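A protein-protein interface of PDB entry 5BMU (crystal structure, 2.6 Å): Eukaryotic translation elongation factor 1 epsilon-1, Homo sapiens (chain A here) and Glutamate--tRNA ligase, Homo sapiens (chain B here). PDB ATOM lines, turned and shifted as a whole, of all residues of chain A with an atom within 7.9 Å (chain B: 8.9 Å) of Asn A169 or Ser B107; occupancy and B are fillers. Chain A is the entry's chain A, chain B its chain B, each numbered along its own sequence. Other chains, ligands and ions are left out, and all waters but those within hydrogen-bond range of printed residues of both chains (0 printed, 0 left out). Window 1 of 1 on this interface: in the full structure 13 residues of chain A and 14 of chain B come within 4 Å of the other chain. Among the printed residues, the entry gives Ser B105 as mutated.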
ATOM      1  N   TYR A 141     -36.094 -20.681  19.396  1.00  0.00           N
ATOM      2  CA  TYR A 141     -34.967 -20.946  20.285  1.00  0.00           C
ATOM      3  C   TYR A 141     -33.697 -21.268  19.480  1.00  0.00           C
ATOM      4  O   TYR A 141     -32.976 -22.188  19.786  1.00  0.00           O
ATOM      5  CB  TYR A 141     -35.324 -22.074  21.257  1.00  0.00           C
ATOM      6  CG  TYR A 141     -36.459 -21.755  22.216  1.00  0.00           C
ATOM      7  CD1 TYR A 141     -36.507 -20.540  22.918  1.00  0.00           C
ATOM      8  CD2 TYR A 141     -37.475 -22.673  22.445  1.00  0.00           C
ATOM      9  CE1 TYR A 141     -37.543 -20.256  23.792  1.00  0.00           C
ATOM     10  CE2 TYR A 141     -38.509 -22.388  23.313  1.00  0.00           C
ATOM     11  CZ  TYR A 141     -38.534 -21.185  23.981  1.00  0.00           C
ATOM     12  OH  TYR A 141     -39.559 -20.923  24.844  1.00  0.00           O
ATOM     13  N   LEU A 142     -33.426 -20.446  18.474  1.00  0.00           N
ATOM     14  CA  LEU A 142     -32.405 -20.709  17.432  1.00  0.00           C
ATOM     15  C   LEU A 142     -31.011 -21.193  17.925  1.00  0.00           C
ATOM     16  O   LEU A 142     -30.430 -22.117  17.349  1.00  0.00           O
ATOM     17  CB  LEU A 142     -32.226 -19.428  16.623  1.00  0.00           C
ATOM     18  CG  LEU A 142     -31.366 -19.451  15.379  1.00  0.00           C
ATOM     19  CD1 LEU A 142     -32.173 -20.024  14.225  1.00  0.00           C
ATOM     20  CD2 LEU A 142     -30.866 -18.054  15.064  1.00  0.00           C
ATOM     21  N   ASN A 143     -30.481 -20.550  18.964  1.00  0.00           N
ATOM     22  CA  ASN A 143     -29.140 -20.849  19.452  1.00  0.00           C
ATOM     23  C   ASN A 143     -29.080 -22.197  20.208  1.00  0.00           C
ATOM     24  O   ASN A 143     -28.028 -22.854  20.267  1.00  0.00           O
ATOM     25  CB  ASN A 143     -28.626 -19.710  20.341  1.00  0.00           C
ATOM     26  CG  ASN A 143     -28.613 -18.349  19.628  1.00  0.00           C
ATOM     27  OD1 ASN A 143     -27.859 -18.124  18.673  1.00  0.00           O
ATOM     28  ND2 ASN A 143     -29.435 -17.430  20.107  1.00  0.00           N
ATOM     29  N   VAL A 144     -30.217 -22.557  20.807  1.00  0.00           N
ATOM     30  CA  VAL A 144     -30.421 -23.817  21.498  1.00  0.00           C
ATOM     31  C   VAL A 144     -30.419 -24.952  20.492  1.00  0.00           C
ATOM     32  O   VAL A 144     -29.697 -25.944  20.656  1.00  0.00           O
ATOM     33  CB  VAL A 144     -31.774 -23.814  22.259  1.00  0.00           C
ATOM     34  CG1 VAL A 144     -32.187 -25.219  22.697  1.00  0.00           C
ATOM     35  CG2 VAL A 144     -31.702 -22.856  23.443  1.00  0.00           C
ATOM     36  N   SER A 145     -31.111 -24.724  19.421  1.00  0.00           N
ATOM     37  CA  SER A 145     -31.208 -25.639  18.371  1.00  0.00           C
ATOM     38  C   SER A 145     -29.876 -25.937  17.796  1.00  0.00           C
ATOM     39  O   SER A 145     -29.576 -27.049  17.454  1.00  0.00           O
ATOM     40  CB  SER A 145     -32.038 -25.022  17.286  1.00  0.00           C
ATOM     41  OG  SER A 145     -33.347 -25.254  17.482  1.00  0.00           O
ATOM     42  N   ARG A 146     -29.096 -24.905  17.637  1.00  0.00           N
ATOM     43  CA  ARG A 146     -27.814 -25.039  17.060  1.00  0.00           C
ATOM     44  C   ARG A 146     -26.853 -25.793  17.899  1.00  0.00           C
ATOM     45  O   ARG A 146     -26.273 -26.735  17.434  1.00  0.00           O
ATOM     46  CB  ARG A 146     -27.302 -23.698  16.653  1.00  0.00           C
ATOM     47  CG  ARG A 146     -25.985 -23.729  15.963  1.00  0.00           C
ATOM     48  CD  ARG A 146     -25.165 -22.556  16.246  1.00  0.00           C
ATOM     49  NE  ARG A 146     -24.557 -22.641  17.536  1.00  0.00           N
ATOM     50  CZ  ARG A 146     -24.913 -21.908  18.548  1.00  0.00           C
ATOM     51  NH1 ARG A 146     -25.855 -21.058  18.416  1.00  0.00           N
ATOM     52  NH2 ARG A 146     -24.342 -22.013  19.677  1.00  0.00           N
ATOM     53  N   TRP A 147     -26.794 -25.444  19.160  1.00  0.00           N
ATOM     54  CA  TRP A 147     -25.957 -26.089  20.097  1.00  0.00           C
ATOM     55  C   TRP A 147     -26.324 -27.563  20.242  1.00  0.00           C
ATOM     56  O   TRP A 147     -25.473 -28.372  20.277  1.00  0.00           O
ATOM     57  CB  TRP A 147     -25.992 -25.350  21.455  1.00  0.00           C
ATOM     58  CG  TRP A 147     -25.462 -26.102  22.613  1.00  0.00           C
ATOM     59  CD1 TRP A 147     -24.201 -26.205  22.968  1.00  0.00           C
ATOM     60  CD2 TRP A 147     -26.183 -26.879  23.523  1.00  0.00           C
ATOM     61  NE1 TRP A 147     -24.058 -26.964  24.013  1.00  0.00           N
ATOM     62  CE2 TRP A 147     -25.272 -27.422  24.384  1.00  0.00           C
ATOM     63  CE3 TRP A 147     -27.523 -27.186  23.688  1.00  0.00           C
ATOM     64  CZ2 TRP A 147     -25.636 -28.245  25.409  1.00  0.00           C
ATOM     65  CZ3 TRP A 147     -27.865 -27.973  24.671  1.00  0.00           C
ATOM     66  CH2 TRP A 147     -26.942 -28.498  25.539  1.00  0.00           C
ATOM     67  N   PHE A 166     -33.421 -30.730  12.402  1.00  0.00           N
ATOM     68  CA  PHE A 166     -33.041 -29.312  12.486  1.00  0.00           C
ATOM     69  C   PHE A 166     -32.732 -28.673  11.124  1.00  0.00           C
ATOM     70  O   PHE A 166     -31.571 -28.674  10.668  1.00  0.00           O
ATOM     71  CB  PHE A 166     -31.817 -29.163  13.384  1.00  0.00           C
ATOM     72  CG  PHE A 166     -32.094 -29.384  14.835  1.00  0.00           C
ATOM     73  CD1 PHE A 166     -32.840 -28.464  15.566  1.00  0.00           C
ATOM     74  CD2 PHE A 166     -31.579 -30.505  15.487  1.00  0.00           C
ATOM     75  CE1 PHE A 166     -33.078 -28.665  16.916  1.00  0.00           C
ATOM     76  CE2 PHE A 166     -31.817 -30.711  16.830  1.00  0.00           C
ATOM     77  CZ  PHE A 166     -32.572 -29.794  17.548  1.00  0.00           C
ATOM     78  N   ILE A 167     -33.772 -28.082  10.522  1.00  0.00           N
ATOM     79  CA  ILE A 167     -33.732 -27.555   9.140  1.00  0.00           C
ATOM     80  C   ILE A 167     -32.460 -26.718   8.858  1.00  0.00           C
ATOM     81  O   ILE A 167     -32.213 -25.695   9.488  1.00  0.00           O
ATOM     82  CB  ILE A 167     -35.034 -26.792   8.779  1.00  0.00           C
ATOM     83  CG1 ILE A 167     -35.213 -25.493   9.597  1.00  0.00           C
ATOM     84  CG2 ILE A 167     -36.256 -27.715   8.909  1.00  0.00           C
ATOM     85  CD1 ILE A 167     -35.098 -24.228   8.759  1.00  0.00           C
ATOM     86  N   LYS A 168     -31.649 -27.200   7.924  1.00  0.00           N
ATOM     87  CA  LYS A 168     -30.212 -26.877   7.867  1.00  0.00           C
ATOM     88  C   LYS A 168     -29.822 -25.429   7.584  1.00  0.00           C
ATOM     89  O   LYS A 168     -28.859 -24.941   8.162  1.00  0.00           O
ATOM     90  CB  LYS A 168     -29.512 -27.747   6.805  1.00  0.00           C
ATOM     91  CG  LYS A 168     -29.224 -29.186   7.219  1.00  0.00           C
ATOM     92  CD  LYS A 168     -27.962 -29.723   6.551  1.00  0.00           C
ATOM     93  CE  LYS A 168     -28.018 -29.635   5.035  1.00  0.00           C
ATOM     94  NZ  LYS A 168     -26.698 -29.803   4.390  1.00  0.00           N
ATOM     95  N   ASN A 169     -30.562 -24.771   6.695  1.00  0.00           N
ATOM     96  CA  ASN A 169     -30.110 -23.566   5.960  1.00  0.00           C
ATOM     97  C   ASN A 169     -29.062 -23.881   4.902  1.00  0.00           C
ATOM     98  O   ASN A 169     -29.114 -23.350   3.795  1.00  0.00           O
ATOM     99  CB  ASN A 169     -29.576 -22.466   6.877  1.00  0.00           C
ATOM    100  CG  ASN A 169     -30.462 -22.217   8.063  1.00  0.00           C
ATOM    101  OD1 ASN A 169     -30.015 -22.321   9.212  1.00  0.00           O
ATOM    102  ND2 ASN A 169     -31.735 -21.921   7.800  1.00  0.00           N
ATOM    103  N   GLU B  77     -20.845 -28.506  -1.445  1.00  0.00           N
ATOM    104  CA  GLU B  77     -20.824 -27.365  -0.518  1.00  0.00           C
ATOM    105  C   GLU B  77     -19.481 -26.705  -0.294  1.00  0.00           C
ATOM    106  O   GLU B  77     -19.362 -25.486  -0.285  1.00  0.00           O
ATOM    107  CB  GLU B  77     -21.208 -27.826   0.864  1.00  0.00           C
ATOM    108  CG  GLU B  77     -22.658 -28.064   1.120  1.00  0.00           C
ATOM    109  CD  GLU B  77     -22.880 -28.090   2.596  1.00  0.00           C
ATOM    110  OE1 GLU B  77     -22.279 -27.203   3.271  1.00  0.00           O
ATOM    111  OE2 GLU B  77     -23.607 -28.984   3.062  1.00  0.00           O
ATOM    112  N   HIS B  80     -18.695 -24.893  -3.299  1.00  0.00           N
ATOM    113  CA  HIS B  80     -19.610 -23.753  -3.244  1.00  0.00           C
ATOM    114  C   HIS B  80     -19.058 -22.623  -2.383  1.00  0.00           C
ATOM    115  O   HIS B  80     -19.046 -21.479  -2.833  1.00  0.00           O
ATOM    116  CB  HIS B  80     -20.970 -24.173  -2.659  1.00  0.00           C
ATOM    117  CG  HIS B  80     -22.121 -23.314  -3.085  1.00  0.00           C
ATOM    118  ND1 HIS B  80     -21.974 -22.077  -3.678  1.00  0.00           N
ATOM    119  CD2 HIS B  80     -23.457 -23.527  -2.984  1.00  0.00           C
ATOM    120  CE1 HIS B  80     -23.170 -21.579  -3.942  1.00  0.00           C
ATOM    121  NE2 HIS B  80     -24.086 -22.438  -3.526  1.00  0.00           N
ATOM    122  N   TRP B  81     -18.617 -22.957  -1.162  1.00  0.00           N
ATOM    123  CA  TRP B  81     -18.093 -21.964  -0.219  1.00  0.00           C
ATOM    124  C   TRP B  81     -16.845 -21.257  -0.732  1.00  0.00           C
ATOM    125  O   TRP B  81     -16.687 -20.048  -0.525  1.00  0.00           O
ATOM    126  CB  TRP B  81     -17.843 -22.561   1.185  1.00  0.00           C
ATOM    127  CG  TRP B  81     -19.127 -22.738   1.941  1.00  0.00           C
ATOM    128  CD1 TRP B  81     -19.721 -23.907   2.301  1.00  0.00           C
ATOM    129  CD2 TRP B  81     -20.002 -21.692   2.381  1.00  0.00           C
ATOM    130  NE1 TRP B  81     -20.897 -23.660   2.941  1.00  0.00           N
ATOM    131  CE2 TRP B  81     -21.102 -22.308   3.000  1.00  0.00           C
ATOM    132  CE3 TRP B  81     -19.940 -20.288   2.340  1.00  0.00           C
ATOM    133  CZ2 TRP B  81     -22.148 -21.573   3.572  1.00  0.00           C
ATOM    134  CZ3 TRP B  81     -20.986 -19.555   2.893  1.00  0.00           C
ATOM    135  CH2 TRP B  81     -22.075 -20.197   3.498  1.00  0.00           C
ATOM    136  N   ASN B 100     -25.438 -11.248   5.086  1.00  0.00           N
ATOM    137  CA  ASN B 100     -26.732 -11.730   5.553  1.00  0.00           C
ATOM    138  C   ASN B 100     -26.770 -13.245   5.361  1.00  0.00           C
ATOM    139  O   ASN B 100     -27.067 -13.978   6.294  1.00  0.00           O
ATOM    140  CB  ASN B 100     -27.897 -11.080   4.787  1.00  0.00           C
ATOM    141  CG  ASN B 100     -29.247 -11.345   5.430  1.00  0.00           C
ATOM    142  OD1 ASN B 100     -29.333 -11.671   6.618  1.00  0.00           O
ATOM    143  ND2 ASN B 100     -30.310 -11.187   4.656  1.00  0.00           N
ATOM    144  N   GLU B 101     -26.456 -13.681   4.137  1.00  0.00           N
ATOM    145  CA  GLU B 101     -26.409 -15.099   3.771  1.00  0.00           C
ATOM    146  C   GLU B 101     -25.450 -15.938   4.633  1.00  0.00           C
ATOM    147  O   GLU B 101     -25.769 -17.084   4.950  1.00  0.00           O
ATOM    148  CB  GLU B 101     -26.069 -15.277   2.275  1.00  0.00           C
ATOM    149  CG  GLU B 101     -27.277 -15.401   1.357  1.00  0.00           C
ATOM    150  CD  GLU B 101     -26.885 -15.743  -0.075  1.00  0.00           C
ATOM    151  OE1 GLU B 101     -26.311 -14.861  -0.750  1.00  0.00           O
ATOM    152  OE2 GLU B 101     -27.133 -16.892  -0.516  1.00  0.00           O
ATOM    153  N   LEU B 102     -24.296 -15.378   5.003  1.00  0.00           N
ATOM    154  CA  LEU B 102     -23.331 -16.083   5.856  1.00  0.00           C
ATOM    155  C   LEU B 102     -23.780 -16.103   7.323  1.00  0.00           C
ATOM    156  O   LEU B 102     -23.543 -17.055   8.044  1.00  0.00           O
ATOM    157  CB  LEU B 102     -21.940 -15.445   5.747  1.00  0.00           C
ATOM    158  CG  LEU B 102     -20.837 -15.968   6.680  1.00  0.00           C
ATOM    159  CD1 LEU B 102     -20.558 -17.456   6.454  1.00  0.00           C
ATOM    160  CD2 LEU B 102     -19.583 -15.146   6.486  1.00  0.00           C
ATOM    161  N   ASN B 103     -24.378 -15.013   7.771  1.00  0.00           N
ATOM    162  CA  ASN B 103     -25.113 -15.004   9.005  1.00  0.00           C
ATOM    163  C   ASN B 103     -26.314 -15.979   9.031  1.00  0.00           C
ATOM    164  O   ASN B 103     -26.641 -16.538  10.086  1.00  0.00           O
ATOM    165  CB  ASN B 103     -25.613 -13.606   9.261  1.00  0.00           C
ATOM    166  CG  ASN B 103     -26.271 -13.461  10.623  1.00  0.00           C
ATOM    167  OD1 ASN B 103     -25.634 -13.677  11.667  1.00  0.00           O
ATOM    168  ND2 ASN B 103     -27.540 -13.077  10.623  1.00  0.00           N
ATOM    169  N   HIS B 104     -26.957 -16.168   7.885  1.00  0.00           N
ATOM    170  CA  HIS B 104     -28.221 -16.863   7.822  1.00  0.00           C
ATOM    171  C   HIS B 104     -28.028 -18.357   7.859  1.00  0.00           C
ATOM    172  O   HIS B 104     -28.817 -19.045   8.521  1.00  0.00           O
ATOM    173  CB  HIS B 104     -29.038 -16.501   6.554  1.00  0.00           C
ATOM    174  CG  HIS B 104     -30.271 -17.337   6.403  1.00  0.00           C
ATOM    175  ND1 HIS B 104     -30.389 -18.325   5.448  1.00  0.00           N
ATOM    176  CD2 HIS B 104     -31.387 -17.417   7.166  1.00  0.00           C
ATOM    177  CE1 HIS B 104     -31.554 -18.934   5.589  1.00  0.00           C
ATOM    178  NE2 HIS B 104     -32.175 -18.405   6.628  1.00  0.00           N
ATOM    179  N   SER B 105     -27.037 -18.851   7.101  1.00  0.00           N
ATOM    180  CA  SER B 105     -26.755 -20.289   7.029  1.00  0.00           C
ATOM    181  C   SER B 105     -25.917 -20.783   8.219  1.00  0.00           C
ATOM    182  O   SER B 105     -26.031 -21.947   8.597  1.00  0.00           O
ATOM    183  CB  SER B 105     -26.178 -20.738   5.656  1.00  0.00           C
ATOM    184  OG  SER B 105     -25.221 -19.853   5.057  1.00  0.00           O
ATOM    185  N   LEU B 106     -25.119 -19.891   8.819  1.00  0.00           N
ATOM    186  CA  LEU B 106     -24.456 -20.169  10.112  1.00  0.00           C
ATOM    187  C   LEU B 106     -25.398 -20.265  11.324  1.00  0.00           C
ATOM    188  O   LEU B 106     -24.931 -20.633  12.388  1.00  0.00           O
ATOM    189  CB  LEU B 106     -23.357 -19.143  10.438  1.00  0.00           C
ATOM    190  CG  LEU B 106     -21.985 -19.347   9.804  1.00  0.00           C
ATOM    191  CD1 LEU B 106     -21.087 -18.138  10.006  1.00  0.00           C
ATOM    192  CD2 LEU B 106     -21.307 -20.584  10.358  1.00  0.00           C
ATOM    193  N   SER B 107     -26.690 -19.944  11.181  1.00  0.00           N
ATOM    194  CA  SER B 107     -27.646 -19.968  12.305  1.00  0.00           C
ATOM    195  C   SER B 107     -27.694 -21.309  13.030  1.00  0.00           C
ATOM    196  O   SER B 107     -27.559 -21.377  14.264  1.00  0.00           O
ATOM    197  CB  SER B 107     -29.069 -19.661  11.826  1.00  0.00           C
ATOM    198  OG  SER B 107     -29.107 -18.615  10.892  1.00  0.00           O
ATOM    199  N   LEU B 108     -27.899 -22.369  12.260  1.00  0.00           N
ATOM    200  CA  LEU B 108     -27.975 -23.717  12.819  1.00  0.00           C
ATOM    201  C   LEU B 108     -26.726 -24.573  12.591  1.00  0.00           C
ATOM    202  O   LEU B 108     -26.750 -25.749  12.892  1.00  0.00           O
ATOM    203  CB  LEU B 108     -29.220 -24.431  12.307  1.00  0.00           C
ATOM    204  CG  LEU B 108     -30.441 -24.345  13.215  1.00  0.00           C
ATOM    205  CD1 LEU B 108     -31.013 -22.941  13.245  1.00  0.00           C
ATOM    206  CD2 LEU B 108     -31.499 -25.331  12.751  1.00  0.00           C
ATOM    207  N   ARG B 109     -25.626 -23.970  12.158  1.00  0.00           N
ATOM    208  CA  ARG B 109     -24.400 -24.689  11.860  1.00  0.00           C
ATOM    209  C   ARG B 109     -23.203 -24.188  12.741  1.00  0.00           C
ATOM    210  O   ARG B 109     -22.948 -22.980  12.870  1.00  0.00           O
ATOM    211  CB  ARG B 109     -24.107 -24.581  10.359  1.00  0.00           C
ATOM    212  CG  ARG B 109     -25.303 -24.905   9.451  1.00  0.00           C
ATOM    213  CD  ARG B 109     -24.982 -24.781   7.965  1.00  0.00           C
ATOM    214  NE  ARG B 109     -24.420 -26.017   7.420  1.00  0.00           N
ATOM    215  CZ  ARG B 109     -24.855 -26.679   6.336  1.00  0.00           C
ATOM    216  NH1 ARG B 109     -25.875 -26.245   5.592  1.00  0.00           N
ATOM    217  NH2 ARG B 109     -24.229 -27.800   5.973  1.00  0.00           N
ATOM    218  N   THR B 110     -22.489 -25.139  13.347  1.00  0.00           N
ATOM    219  CA  THR B 110     -21.292 -24.855  14.164  1.00  0.00           C
ATOM    220  C   THR B 110     -20.148 -24.675  13.193  1.00  0.00           C
ATOM    221  O   THR B 110     -19.370 -23.712  13.262  1.00  0.00           O
ATOM    222  CB  THR B 110     -21.015 -26.014  15.154  1.00  0.00           C
ATOM    223  OG1 THR B 110     -22.094 -26.091  16.081  1.00  0.00           O
ATOM    224  CG2 THR B 110     -19.735 -25.830  15.945  1.00  0.00           C
ATOM    225  N   TYR B 111     -20.055 -25.623  12.277  1.00  0.00           N
ATOM    226  CA  TYR B 111     -19.240 -25.461  11.075  1.00  0.00           C
ATOM    227  C   TYR B 111     -20.112 -25.281   9.854  1.00  0.00           C
ATOM    228  O   TYR B 111     -21.229 -25.748   9.824  1.00  0.00           O
ATOM    229  CB  TYR B 111     -18.340 -26.664  10.911  1.00  0.00           C
ATOM    230  CG  TYR B 111     -17.419 -26.849  12.085  1.00  0.00           C
ATOM    231  CD1 TYR B 111     -16.190 -26.220  12.124  1.00  0.00           C
ATOM    232  CD2 TYR B 111     -17.781 -27.670  13.159  1.00  0.00           C
ATOM    233  CE1 TYR B 111     -15.341 -26.386  13.207  1.00  0.00           C
ATOM    234  CE2 TYR B 111     -16.933 -27.867  14.247  1.00  0.00           C
ATOM    235  CZ  TYR B 111     -15.720 -27.216  14.273  1.00  0.00           C
ATOM    236  OH  TYR B 111     -14.893 -27.386  15.352  1.00  0.00           O
ATOM    237  N   LEU B 112     -19.583 -24.695   8.822  1.00  0.00           N
ATOM    238  CA  LEU B 112     -20.258 -24.531   7.562  1.00  0.00           C
ATOM    239  C   LEU B 112     -20.580 -25.887   6.972  1.00  0.00           C
ATOM    240  O   LEU B 112     -21.452 -26.057   6.232  1.00  0.00           O
ATOM    241  CB  LEU B 112     -19.353 -23.752   6.638  1.00  0.00           C
ATOM    242  CG  LEU B 112     -19.268 -22.256   6.774  1.00  0.00           C
ATOM    243  CD1 LEU B 112     -18.204 -21.633   5.956  1.00  0.00           C
ATOM    244  CD2 LEU B 112     -20.569 -21.596   6.540  1.00  0.00           C
ATOM    245  N   VAL B 145     -24.497 -11.724  14.476  1.00  0.00           N
ATOM    246  CA  VAL B 145     -24.146 -12.487  15.712  1.00  0.00           C
ATOM    247  C   VAL B 145     -23.615 -13.925  15.466  1.00  0.00           C
ATOM    248  O   VAL B 145     -22.667 -14.357  16.089  1.00  0.00           O
ATOM    249  CB  VAL B 145     -25.306 -12.529  16.747  1.00  0.00           C
ATOM    250  CG1 VAL B 145     -25.717 -11.123  17.165  1.00  0.00           C
ATOM    251  CG2 VAL B 145     -26.503 -13.330  16.226  1.00  0.00           C
ATOM    252  N   HIS B 146     -24.219 -14.639  14.539  1.00  0.00           N
ATOM    253  CA  HIS B 146     -23.765 -15.983  14.182  1.00  0.00           C
ATOM    254  C   HIS B 146     -22.390 -15.998  13.455  1.00  0.00           C
ATOM    255  O   HIS B 146     -21.584 -16.912  13.680  1.00  0.00           O
ATOM    256  CB  HIS B 146     -24.820 -16.675  13.322  1.00  0.00           C
ATOM    257  CG  HIS B 146     -26.222 -16.440  13.789  1.00  0.00           C
ATOM    258  ND1 HIS B 146     -26.697 -16.933  14.979  1.00  0.00           N
ATOM    259  CD2 HIS B 146     -27.251 -15.765  13.227  1.00  0.00           C
ATOM    260  CE1 HIS B 146     -27.952 -16.568  15.137  1.00  0.00           C
ATOM    261  NE2 HIS B 146     -28.314 -15.857  14.086  1.00  0.00           N
ATOM    262  N   VAL B 147     -22.118 -14.995  12.608  1.00  0.00           N
ATOM    263  CA  VAL B 147     -20.789 -14.892  11.956  1.00  0.00           C
ATOM    264  C   VAL B 147     -19.696 -14.572  12.983  1.00  0.00           C
ATOM    265  O   VAL B 147     -18.540 -14.895  12.794  1.00  0.00           O
ATOM    266  CB  VAL B 147     -20.749 -13.843  10.809  1.00  0.00           C
ATOM    267  CG1 VAL B 147     -19.371 -13.806  10.154  1.00  0.00           C
ATOM    268  CG2 VAL B 147     -21.803 -14.139   9.770  1.00  0.00           C
ATOM    269  N   ARG B 149     -19.642 -15.470  16.529  1.00  0.00           N
ATOM    270  CA  ARG B 149     -19.277 -16.641  17.302  1.00  0.00           C
ATOM    271  C   ARG B 149     -18.410 -17.577  16.456  1.00  0.00           C
ATOM    272  O   ARG B 149     -17.457 -18.145  16.952  1.00  0.00           O
ATOM    273  CB  ARG B 149     -20.514 -17.365  17.820  1.00  0.00           C
ATOM    274  CG  ARG B 149     -21.409 -17.949  16.740  1.00  0.00           C
ATOM    275  CD  ARG B 149     -22.408 -18.913  17.331  1.00  0.00           C
ATOM    276  NE  ARG B 149     -23.531 -19.114  16.418  1.00  0.00           N
ATOM    277  CZ  ARG B 149     -23.536 -19.910  15.344  1.00  0.00           C
ATOM    278  NH1 ARG B 149     -22.478 -20.647  14.983  1.00  0.00           N
ATOM    279  NH2 ARG B 149     -24.649 -19.983  14.631  1.00  0.00           N
ATOM    280  N   TRP B 150     -18.757 -17.680  15.175  1.00  0.00           N
ATOM    281  CA  TRP B 150     -18.163 -18.609  14.246  1.00  0.00           C
ATOM    282  C   TRP B 150     -16.727 -18.148  13.982  1.00  0.00           C
ATOM    283  O   TRP B 150     -15.784 -18.929  14.150  1.00  0.00           O
ATOM    284  CB  TRP B 150     -19.046 -18.679  12.976  1.00  0.00           C
ATOM    285  CG  TRP B 150     -18.454 -19.400  11.856  1.00  0.00           C
ATOM    286  CD1 TRP B 150     -18.482 -20.740  11.632  1.00  0.00           C
ATOM    287  CD2 TRP B 150     -17.714 -18.832  10.789  1.00  0.00           C
ATOM    288  NE1 TRP B 150     -17.803 -21.046  10.482  1.00  0.00           N
ATOM    289  CE2 TRP B 150     -17.302 -19.892   9.955  1.00  0.00           C
ATOM    290  CE3 TRP B 150     -17.346 -17.529  10.454  1.00  0.00           C
ATOM    291  CZ2 TRP B 150     -16.545 -19.687   8.811  1.00  0.00           C
ATOM    292  CZ3 TRP B 150     -16.588 -17.332   9.304  1.00  0.00           C
ATOM    293  CH2 TRP B 150     -16.198 -18.401   8.503  1.00  0.00           C
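The side-chain carboxylate (OE2) of Glu B77 lies within salt-bridge range of the side-chain amino group (NZ) of Lys A168 (3.5 Å).
The backbone carbonyl oxygen (O) of Asn A143 is in hydrogen-bond range of the guanidinium group (NH1) of Arg A146, 3.4 Å away. OE2 of Glu B77 lies within salt-bridge range of NH2 of Arg B109, at 3.2 Å. The backbone carbonyl oxygen (O) of Glu B101 sits at hydrogen-bond distance from the side-chain hydroxyl (OG) of Ser B105 (2.8 Å). The backbone NH of His B146 lies close to the side-chain amide oxygen of Asn B103 (3.3 Å). O of His B104 sits at hydrogen-bond distance from OG of Ser B107 (2.4 Å). O of Leu B112 sits at hydrogen-bond distance from NE of Arg B109, at 3.2 Å.
Leu A142 touches Ser B107. CD2 of Leu A142 touches CE1 of His B146, 3.3 Å away. CG of Arg A146 touches O of Ser B107, 3.3 Å away. Arg A146 touches Leu B108 (CG to C, 3.6 Å). Arg B109 touches Arg A146 (N to CG, 3.8 Å). Phe A166 touches Leu B108 (CB to CD2, 3.9 Å). Lys A168 touches Arg B109. CB of Asn A169 touches CA of Ser B105, 3.6 Å away. Asn A169 touches Ser B107. Leu B108 touches Asn A169 (N to OD1, 3.7 Å).
Of the printed residues of chain B, Asn A169 touches His B104 (3.6 Å), Ser B105 (3.6 Å), Ser B107 (3.8 Å) and Leu B108 (3.7 Å). Of the printed residues of chain A, Ser B107 touches Leu A142, Arg A146 and Asn A169. Printed residues of chain A within 4 Å of Arg B149: Arg A146. Of the printed residues of chain A, Leu B108 touches Leu A142 (3.3 Å), Arg A146 (3.6 Å), Phe A166 (3.9 Å), Ile A167 (3.4 Å) and Asn A169 (3.7 Å). Printed residues of chain B within 4 Å of Leu A142: Ser B107 (3.9 Å), Leu B108 (3.3 Å) and His B146 (3.3 Å). Asn B103 touches none of the printed residues of chain A. The nearest residue of chain A that does not touch Ser B107 is Asn A143 (5.4 Å). The nearest printed residue of chain A that does not touch Arg B109 is Asn A169 (4.03 Å).
Hydrophobic or aromatic side chains of chain B within 4 Å of the printed part of chain A: His B104, Leu B108 and His B146. Along chain B the printed residues that touch a printed residue of chain A span positions 77 to 149. Among the printed residues, Asp or Glu carboxylates within 4 Å of a Lys or Arg side-chain nitrogen of the other chain: Lys A168 with Glu B77 (3.5 Å).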
